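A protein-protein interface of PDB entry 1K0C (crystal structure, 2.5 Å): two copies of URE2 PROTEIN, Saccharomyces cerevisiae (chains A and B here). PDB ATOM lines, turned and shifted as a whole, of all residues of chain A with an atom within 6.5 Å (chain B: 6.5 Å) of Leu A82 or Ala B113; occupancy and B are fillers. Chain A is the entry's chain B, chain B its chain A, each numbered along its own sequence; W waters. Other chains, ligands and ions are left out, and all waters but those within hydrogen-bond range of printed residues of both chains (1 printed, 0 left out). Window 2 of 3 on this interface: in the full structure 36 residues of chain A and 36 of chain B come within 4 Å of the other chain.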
ATOM      1  N   LEU A  74      19.819  -1.271  26.902  1.00  0.00           N
ATOM      2  CA  LEU A  74      19.325  -2.493  27.522  1.00  0.00           C
ATOM      3  C   LEU A  74      18.621  -3.367  26.519  1.00  0.00           C
ATOM      4  O   LEU A  74      17.981  -2.862  25.603  1.00  0.00           O
ATOM      5  CB  LEU A  74      18.326  -2.163  28.634  1.00  0.00           C
ATOM      6  CG  LEU A  74      17.803  -3.352  29.450  1.00  0.00           C
ATOM      7  CD1 LEU A  74      18.884  -3.834  30.414  1.00  0.00           C
ATOM      8  CD2 LEU A  74      16.570  -2.931  30.233  1.00  0.00           C
ATOM      9  N   ILE A  75      18.737  -4.678  26.678  1.00  0.00           N
ATOM     10  CA  ILE A  75      18.028  -5.582  25.787  1.00  0.00           C
ATOM     11  C   ILE A  75      17.039  -6.415  26.591  1.00  0.00           C
ATOM     12  O   ILE A  75      17.416  -7.186  27.477  1.00  0.00           O
ATOM     13  CB  ILE A  75      18.975  -6.518  25.016  1.00  0.00           C
ATOM     14  CG1 ILE A  75      19.826  -5.702  24.039  1.00  0.00           C
ATOM     15  CG2 ILE A  75      18.162  -7.540  24.235  1.00  0.00           C
ATOM     16  CD1 ILE A  75      20.689  -6.542  23.131  1.00  0.00           C
ATOM     17  N   ASP A  76      15.760  -6.227  26.291  1.00  0.00           N
ATOM     18  CA  ASP A  76      14.706  -6.961  26.967  1.00  0.00           C
ATOM     19  C   ASP A  76      14.443  -8.184  26.107  1.00  0.00           C
ATOM     20  O   ASP A  76      13.633  -8.135  25.177  1.00  0.00           O
ATOM     21  CB  ASP A  76      13.445  -6.101  27.066  1.00  0.00           C
ATOM     22  CG  ASP A  76      12.383  -6.726  27.953  1.00  0.00           C
ATOM     23  OD1 ASP A  76      12.259  -7.973  27.942  1.00  0.00           O
ATOM     24  OD2 ASP A  76      11.667  -5.972  28.649  1.00  0.00           O
ATOM     25  N   HIS A  77      15.147  -9.272  26.419  1.00  0.00           N
ATOM     26  CA  HIS A  77      15.038 -10.530  25.680  1.00  0.00           C
ATOM     27  C   HIS A  77      13.629 -11.106  25.711  1.00  0.00           C
ATOM     28  O   HIS A  77      13.078 -11.482  24.675  1.00  0.00           O
ATOM     29  CB  HIS A  77      16.039 -11.550  26.234  1.00  0.00           C
ATOM     30  CG  HIS A  77      17.470 -11.151  26.042  1.00  0.00           C
ATOM     31  ND1 HIS A  77      18.021 -10.939  24.796  1.00  0.00           N
ATOM     32  CD2 HIS A  77      18.452 -10.884  26.937  1.00  0.00           C
ATOM     33  CE1 HIS A  77      19.279 -10.558  24.930  1.00  0.00           C
ATOM     34  NE2 HIS A  77      19.565 -10.515  26.220  1.00  0.00           N
ATOM     35  N   GLY A  78      13.041 -11.167  26.898  1.00  0.00           N
ATOM     36  CA  GLY A  78      11.692 -11.684  27.011  1.00  0.00           C
ATOM     37  C   GLY A  78      10.718 -10.964  26.092  1.00  0.00           C
ATOM     38  O   GLY A  78       9.601 -11.432  25.878  1.00  0.00           O
ATOM     39  N   MET A  79      11.125  -9.821  25.546  1.00  0.00           N
ATOM     40  CA  MET A  79      10.250  -9.071  24.655  1.00  0.00           C
ATOM     41  C   MET A  79      10.734  -9.064  23.213  1.00  0.00           C
ATOM     42  O   MET A  79      10.662  -8.047  22.524  1.00  0.00           O
ATOM     43  CB  MET A  79      10.063  -7.638  25.163  1.00  0.00           C
ATOM     44  CG  MET A  79       9.054  -7.525  26.289  1.00  0.00           C
ATOM     45  SD  MET A  79       8.735  -5.816  26.795  1.00  0.00           S
ATOM     46  CE  MET A  79       7.602  -5.279  25.516  1.00  0.00           C
ATOM     47  N   ASP A  80      11.220 -10.220  22.766  1.00  0.00           N
ATOM     48  CA  ASP A  80      11.696 -10.392  21.398  1.00  0.00           C
ATOM     49  C   ASP A  80      12.967  -9.587  21.168  1.00  0.00           C
ATOM     50  O   ASP A  80      13.213  -9.066  20.078  1.00  0.00           O
ATOM     51  CB  ASP A  80      10.593  -9.965  20.421  1.00  0.00           C
ATOM     52  CG  ASP A  80      10.780 -10.544  19.031  1.00  0.00           C
ATOM     53  OD1 ASP A  80       9.832 -10.429  18.221  1.00  0.00           O
ATOM     54  OD2 ASP A  80      11.864 -11.106  18.743  1.00  0.00           O
ATOM     55  N   ASN A  81      13.775  -9.504  22.216  1.00  0.00           N
ATOM     56  CA  ASN A  81      15.036  -8.780  22.196  1.00  0.00           C
ATOM     57  C   ASN A  81      14.897  -7.298  21.943  1.00  0.00           C
ATOM     58  O   ASN A  81      15.740  -6.681  21.301  1.00  0.00           O
ATOM     59  CB  ASN A  81      15.995  -9.414  21.191  1.00  0.00           C
ATOM     60  CG  ASN A  81      16.346 -10.833  21.573  1.00  0.00           C
ATOM     61  OD1 ASN A  81      16.367 -11.167  22.762  1.00  0.00           O
ATOM     62  ND2 ASN A  81      16.621 -11.675  20.584  1.00  0.00           N
ATOM     63  N   LEU A  82      13.821  -6.729  22.470  1.00  0.00           N
ATOM     64  CA  LEU A  82      13.582  -5.303  22.339  1.00  0.00           C
ATOM     65  C   LEU A  82      14.809  -4.559  22.872  1.00  0.00           C
ATOM     66  O   LEU A  82      15.395  -4.936  23.890  1.00  0.00           O
ATOM     67  CB  LEU A  82      12.341  -4.896  23.133  1.00  0.00           C
ATOM     68  CG  LEU A  82      12.124  -3.383  23.213  1.00  0.00           C
ATOM     69  CD1 LEU A  82      11.956  -2.810  21.811  1.00  0.00           C
ATOM     70  CD2 LEU A  82      10.914  -3.087  24.075  1.00  0.00           C
ATOM     71  N   SER A  83      15.194  -3.501  22.174  1.00  0.00           N
ATOM     72  CA  SER A  83      16.351  -2.717  22.562  1.00  0.00           C
ATOM     73  C   SER A  83      15.962  -1.325  23.053  1.00  0.00           C
ATOM     74  O   SER A  83      15.354  -0.547  22.318  1.00  0.00           O
ATOM     75  CB  SER A  83      17.290  -2.592  21.367  1.00  0.00           C
ATOM     76  OG  SER A  83      18.344  -1.692  21.638  1.00  0.00           O
ATOM     77  N   ILE A  84      16.298  -1.007  24.297  1.00  0.00           N
ATOM     78  CA  ILE A  84      15.987   0.318  24.806  1.00  0.00           C
ATOM     79  C   ILE A  84      17.273   1.079  25.107  1.00  0.00           C
ATOM     80  O   ILE A  84      18.110   0.609  25.871  1.00  0.00           O
ATOM     81  CB  ILE A  84      15.124   0.272  26.093  1.00  0.00           C
ATOM     82  CG1 ILE A  84      13.855  -0.563  25.864  1.00  0.00           C
ATOM     83  CG2 ILE A  84      14.722   1.700  26.488  1.00  0.00           C
ATOM     84  CD1 ILE A  84      13.926  -1.974  26.402  1.00  0.00           C
ATOM     85  N   HIS A  93      10.811   2.174  30.974  1.00  0.00           N
ATOM     86  CA  HIS A  93      10.413   0.874  30.473  1.00  0.00           C
ATOM     87  C   HIS A  93      10.372  -0.091  31.648  1.00  0.00           C
ATOM     88  O   HIS A  93       9.436  -0.875  31.785  1.00  0.00           O
ATOM     89  CB  HIS A  93      11.399   0.378  29.419  1.00  0.00           C
ATOM     90  CG  HIS A  93      11.051  -0.966  28.856  1.00  0.00           C
ATOM     91  ND1 HIS A  93      11.664  -2.131  29.268  1.00  0.00           N
ATOM     92  CD2 HIS A  93      10.146  -1.330  27.918  1.00  0.00           C
ATOM     93  CE1 HIS A  93      11.154  -3.154  28.604  1.00  0.00           C
ATOM     94  NE2 HIS A  93      10.231  -2.694  27.779  1.00  0.00           N
ATOM     95  N   SER B 109       1.269   5.845  21.725  1.00  0.00           N
ATOM     96  CA  SER B 109       1.095   4.440  21.356  1.00  0.00           C
ATOM     97  C   SER B 109       0.635   3.613  22.559  1.00  0.00           C
ATOM     98  O   SER B 109       0.968   3.923  23.699  1.00  0.00           O
ATOM     99  CB  SER B 109       2.415   3.874  20.817  1.00  0.00           C
ATOM    100  OG  SER B 109       2.282   2.513  20.454  1.00  0.00           O
ATOM    101  N   ASP B 110      -0.128   2.558  22.302  1.00  0.00           N
ATOM    102  CA  ASP B 110      -0.613   1.702  23.374  1.00  0.00           C
ATOM    103  C   ASP B 110       0.259   0.457  23.529  1.00  0.00           C
ATOM    104  O   ASP B 110      -0.065  -0.450  24.297  1.00  0.00           O
ATOM    105  CB  ASP B 110      -2.055   1.285  23.103  1.00  0.00           C
ATOM    106  CG  ASP B 110      -2.247   0.784  21.692  1.00  0.00           C
ATOM    107  OD1 ASP B 110      -1.336   0.091  21.189  1.00  0.00           O
ATOM    108  OD2 ASP B 110      -3.304   1.077  21.089  1.00  0.00           O
ATOM    109  N   ASP B 111       1.360   0.405  22.793  1.00  0.00           N
ATOM    110  CA  ASP B 111       2.264  -0.733  22.885  1.00  0.00           C
ATOM    111  C   ASP B 111       3.519  -0.323  23.646  1.00  0.00           C
ATOM    112  O   ASP B 111       4.270   0.537  23.181  1.00  0.00           O
ATOM    113  CB  ASP B 111       2.640  -1.217  21.489  1.00  0.00           C
ATOM    114  CG  ASP B 111       3.697  -2.295  21.522  1.00  0.00           C
ATOM    115  OD1 ASP B 111       3.419  -3.378  22.079  1.00  0.00           O
ATOM    116  OD2 ASP B 111       4.811  -2.056  20.997  1.00  0.00           O
ATOM    117  N   LEU B 112       3.747  -0.934  24.810  1.00  0.00           N
ATOM    118  CA  LEU B 112       4.914  -0.600  25.629  1.00  0.00           C
ATOM    119  C   LEU B 112       6.223  -0.621  24.838  1.00  0.00           C
ATOM    120  O   LEU B 112       7.145   0.148  25.132  1.00  0.00           O
ATOM    121  CB  LEU B 112       5.020  -1.537  26.848  1.00  0.00           C
ATOM    122  CG  LEU B 112       6.359  -1.504  27.621  1.00  0.00           C
ATOM    123  CD1 LEU B 112       6.667  -0.077  28.100  1.00  0.00           C
ATOM    124  CD2 LEU B 112       6.312  -2.476  28.807  1.00  0.00           C
ATOM    125  N   ALA B 113       6.312  -1.495  23.842  1.00  0.00           N
ATOM    126  CA  ALA B 113       7.522  -1.568  23.027  1.00  0.00           C
ATOM    127  C   ALA B 113       7.702  -0.245  22.280  1.00  0.00           C
ATOM    128  O   ALA B 113       8.793   0.335  22.266  1.00  0.00           O
ATOM    129  CB  ALA B 113       7.430  -2.721  22.037  1.00  0.00           C
ATOM    130  N   ASP B 114       6.620   0.224  21.661  1.00  0.00           N
ATOM    131  CA  ASP B 114       6.642   1.480  20.925  1.00  0.00           C
ATOM    132  C   ASP B 114       6.887   2.656  21.859  1.00  0.00           C
ATOM    133  O   ASP B 114       7.553   3.618  21.487  1.00  0.00           O
ATOM    134  CB  ASP B 114       5.321   1.668  20.183  1.00  0.00           C
ATOM    135  CG  ASP B 114       5.209   0.767  18.973  1.00  0.00           C
ATOM    136  OD1 ASP B 114       4.078   0.573  18.472  1.00  0.00           O
ATOM    137  OD2 ASP B 114       6.264   0.264  18.520  1.00  0.00           O
ATOM    138  N   GLN B 115       6.350   2.572  23.071  1.00  0.00           N
ATOM    139  CA  GLN B 115       6.523   3.631  24.058  1.00  0.00           C
ATOM    140  C   GLN B 115       7.987   3.803  24.444  1.00  0.00           C
ATOM    141  O   GLN B 115       8.476   4.926  24.553  1.00  0.00           O
ATOM    142  CB  GLN B 115       5.691   3.341  25.306  1.00  0.00           C
ATOM    143  CG  GLN B 115       4.198   3.332  25.023  1.00  0.00           C
ATOM    144  CD  GLN B 115       3.344   3.122  26.261  1.00  0.00           C
ATOM    145  OE1 GLN B 115       2.121   3.044  26.168  1.00  0.00           O
ATOM    146  NE2 GLN B 115       3.980   3.032  27.423  1.00  0.00           N
ATOM    147  N   SER B 116       8.691   2.693  24.632  1.00  0.00           N
ATOM    148  CA  SER B 116      10.093   2.770  24.997  1.00  0.00           C
ATOM    149  C   SER B 116      10.914   3.410  23.870  1.00  0.00           C
ATOM    150  O   SER B 116      11.847   4.157  24.149  1.00  0.00           O
ATOM    151  CB  SER B 116      10.635   1.378  25.365  1.00  0.00           C
ATOM    152  OG  SER B 116      10.632   0.482  24.264  1.00  0.00           O
ATOM    153  N   GLN B 117      10.566   3.135  22.610  1.00  0.00           N
ATOM    154  CA  GLN B 117      11.275   3.729  21.461  1.00  0.00           C
ATOM    155  C   GLN B 117      11.006   5.227  21.415  1.00  0.00           C
ATOM    156  O   GLN B 117      11.907   6.037  21.191  1.00  0.00           O
ATOM    157  CB  GLN B 117      10.806   3.125  20.128  1.00  0.00           C
ATOM    158  CG  GLN B 117      11.211   1.691  19.892  1.00  0.00           C
ATOM    159  CD  GLN B 117      12.657   1.436  20.257  1.00  0.00           C
ATOM    160  OE1 GLN B 117      12.987   1.210  21.431  1.00  0.00           O
ATOM    161  NE2 GLN B 117      13.539   1.486  19.257  1.00  0.00           N
ATOM    162  N   ILE B 118       9.743   5.589  21.603  1.00  0.00           N
ATOM    163  CA  ILE B 118       9.363   6.984  21.602  1.00  0.00           C
ATOM    164  C   ILE B 118      10.130   7.684  22.712  1.00  0.00           C
ATOM    165  O   ILE B 118      10.700   8.755  22.500  1.00  0.00           O
ATOM    166  CB  ILE B 118       7.867   7.140  21.840  1.00  0.00           C
ATOM    167  CG1 ILE B 118       7.106   6.622  20.616  1.00  0.00           C
ATOM    168  CG2 ILE B 118       7.537   8.603  22.148  1.00  0.00           C
ATOM    169  CD1 ILE B 118       5.592   6.573  20.798  1.00  0.00           C
ATOM    170  N   VAL B 208       9.135   6.370  14.931  1.00  0.00           N
ATOM    171  CA  VAL B 208       8.560   5.184  15.548  1.00  0.00           C
ATOM    172  C   VAL B 208       7.159   4.819  15.080  1.00  0.00           C
ATOM    173  O   VAL B 208       6.257   5.655  15.072  1.00  0.00           O
ATOM    174  CB  VAL B 208       8.498   5.341  17.103  1.00  0.00           C
ATOM    175  CG1 VAL B 208       7.834   4.111  17.750  1.00  0.00           C
ATOM    176  CG2 VAL B 208       9.882   5.555  17.659  1.00  0.00           C
HETATM  177  O   HOH W   1      15.833   0.485  19.367  1.00  0.00           O
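Water W1 bridges NE2 of Gln B117 (2.5 Å) and O of Ser A83 (3.2 Å).
Leu A82 touches just these residues of chain B: Ala B113 (3.9 Å) and Ser B116 (3.6 Å).
Of the printed residues of chain A, Ala B113 touches Leu A82.
Of the printed residues of chain A, Gln B117 touches Ser A83 (3.1 Å).
Printed residues of chain A within 4 Å of Ser B116: Leu A82, Ile A84 and His A93.
Of the printed residues of chain A, Leu B112 touches His A93 (3.7 Å).
The nearest residue of chain B that does not touch Leu A82 is Gln B117 (4.2 Å).
The backbone carbonyl oxygen of Ser A83 sits close to the side-chain amide oxygen of Gln B117 (3.1 Å).
Leu A82 touches Ala B113 (CD2 to CA, 3.9 Å).
CD2 of Leu A82 touches OG of Ser B116, 3.6 Å away.
Ser B116 touches Ile A84.
His A93 touches Leu B112.
CD2 of His A93 touches CB of Ser B116, 3.8 Å away.
The backbone NH of Leu A74 sits at hydrogen-bond distance from the backbone carbonyl oxygen of Ile A84 (2.7 Å).
The backbone NH (N) of Ala B113 sits close to the side-chain carboxylate (OD2) of Asp B111 (3.3 Å).
The side-chain hydroxyl (OG) of Ser B116 sits at hydrogen-bond distance from the backbone carbonyl oxygen (O) of Ala B113 (2.7 Å).
SD of Met A79 is in hydrogen-bond range of NE2 of His A93 (3.6 Å).
The backbone carbonyl oxygen (O) of Leu A82 lies within hydrogen-bond range of the backbone NH (N) of Asp A76 (2.8 Å).
No position is printed for both chains.
Hydrophobic or aromatic side chains of chain B that line the printed part of chain A: Leu B112.
Among the printed residues, no Asp or Glu carboxylate lies within 4 Å of a Lys or Arg side-chain nitrogen of the other chain.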
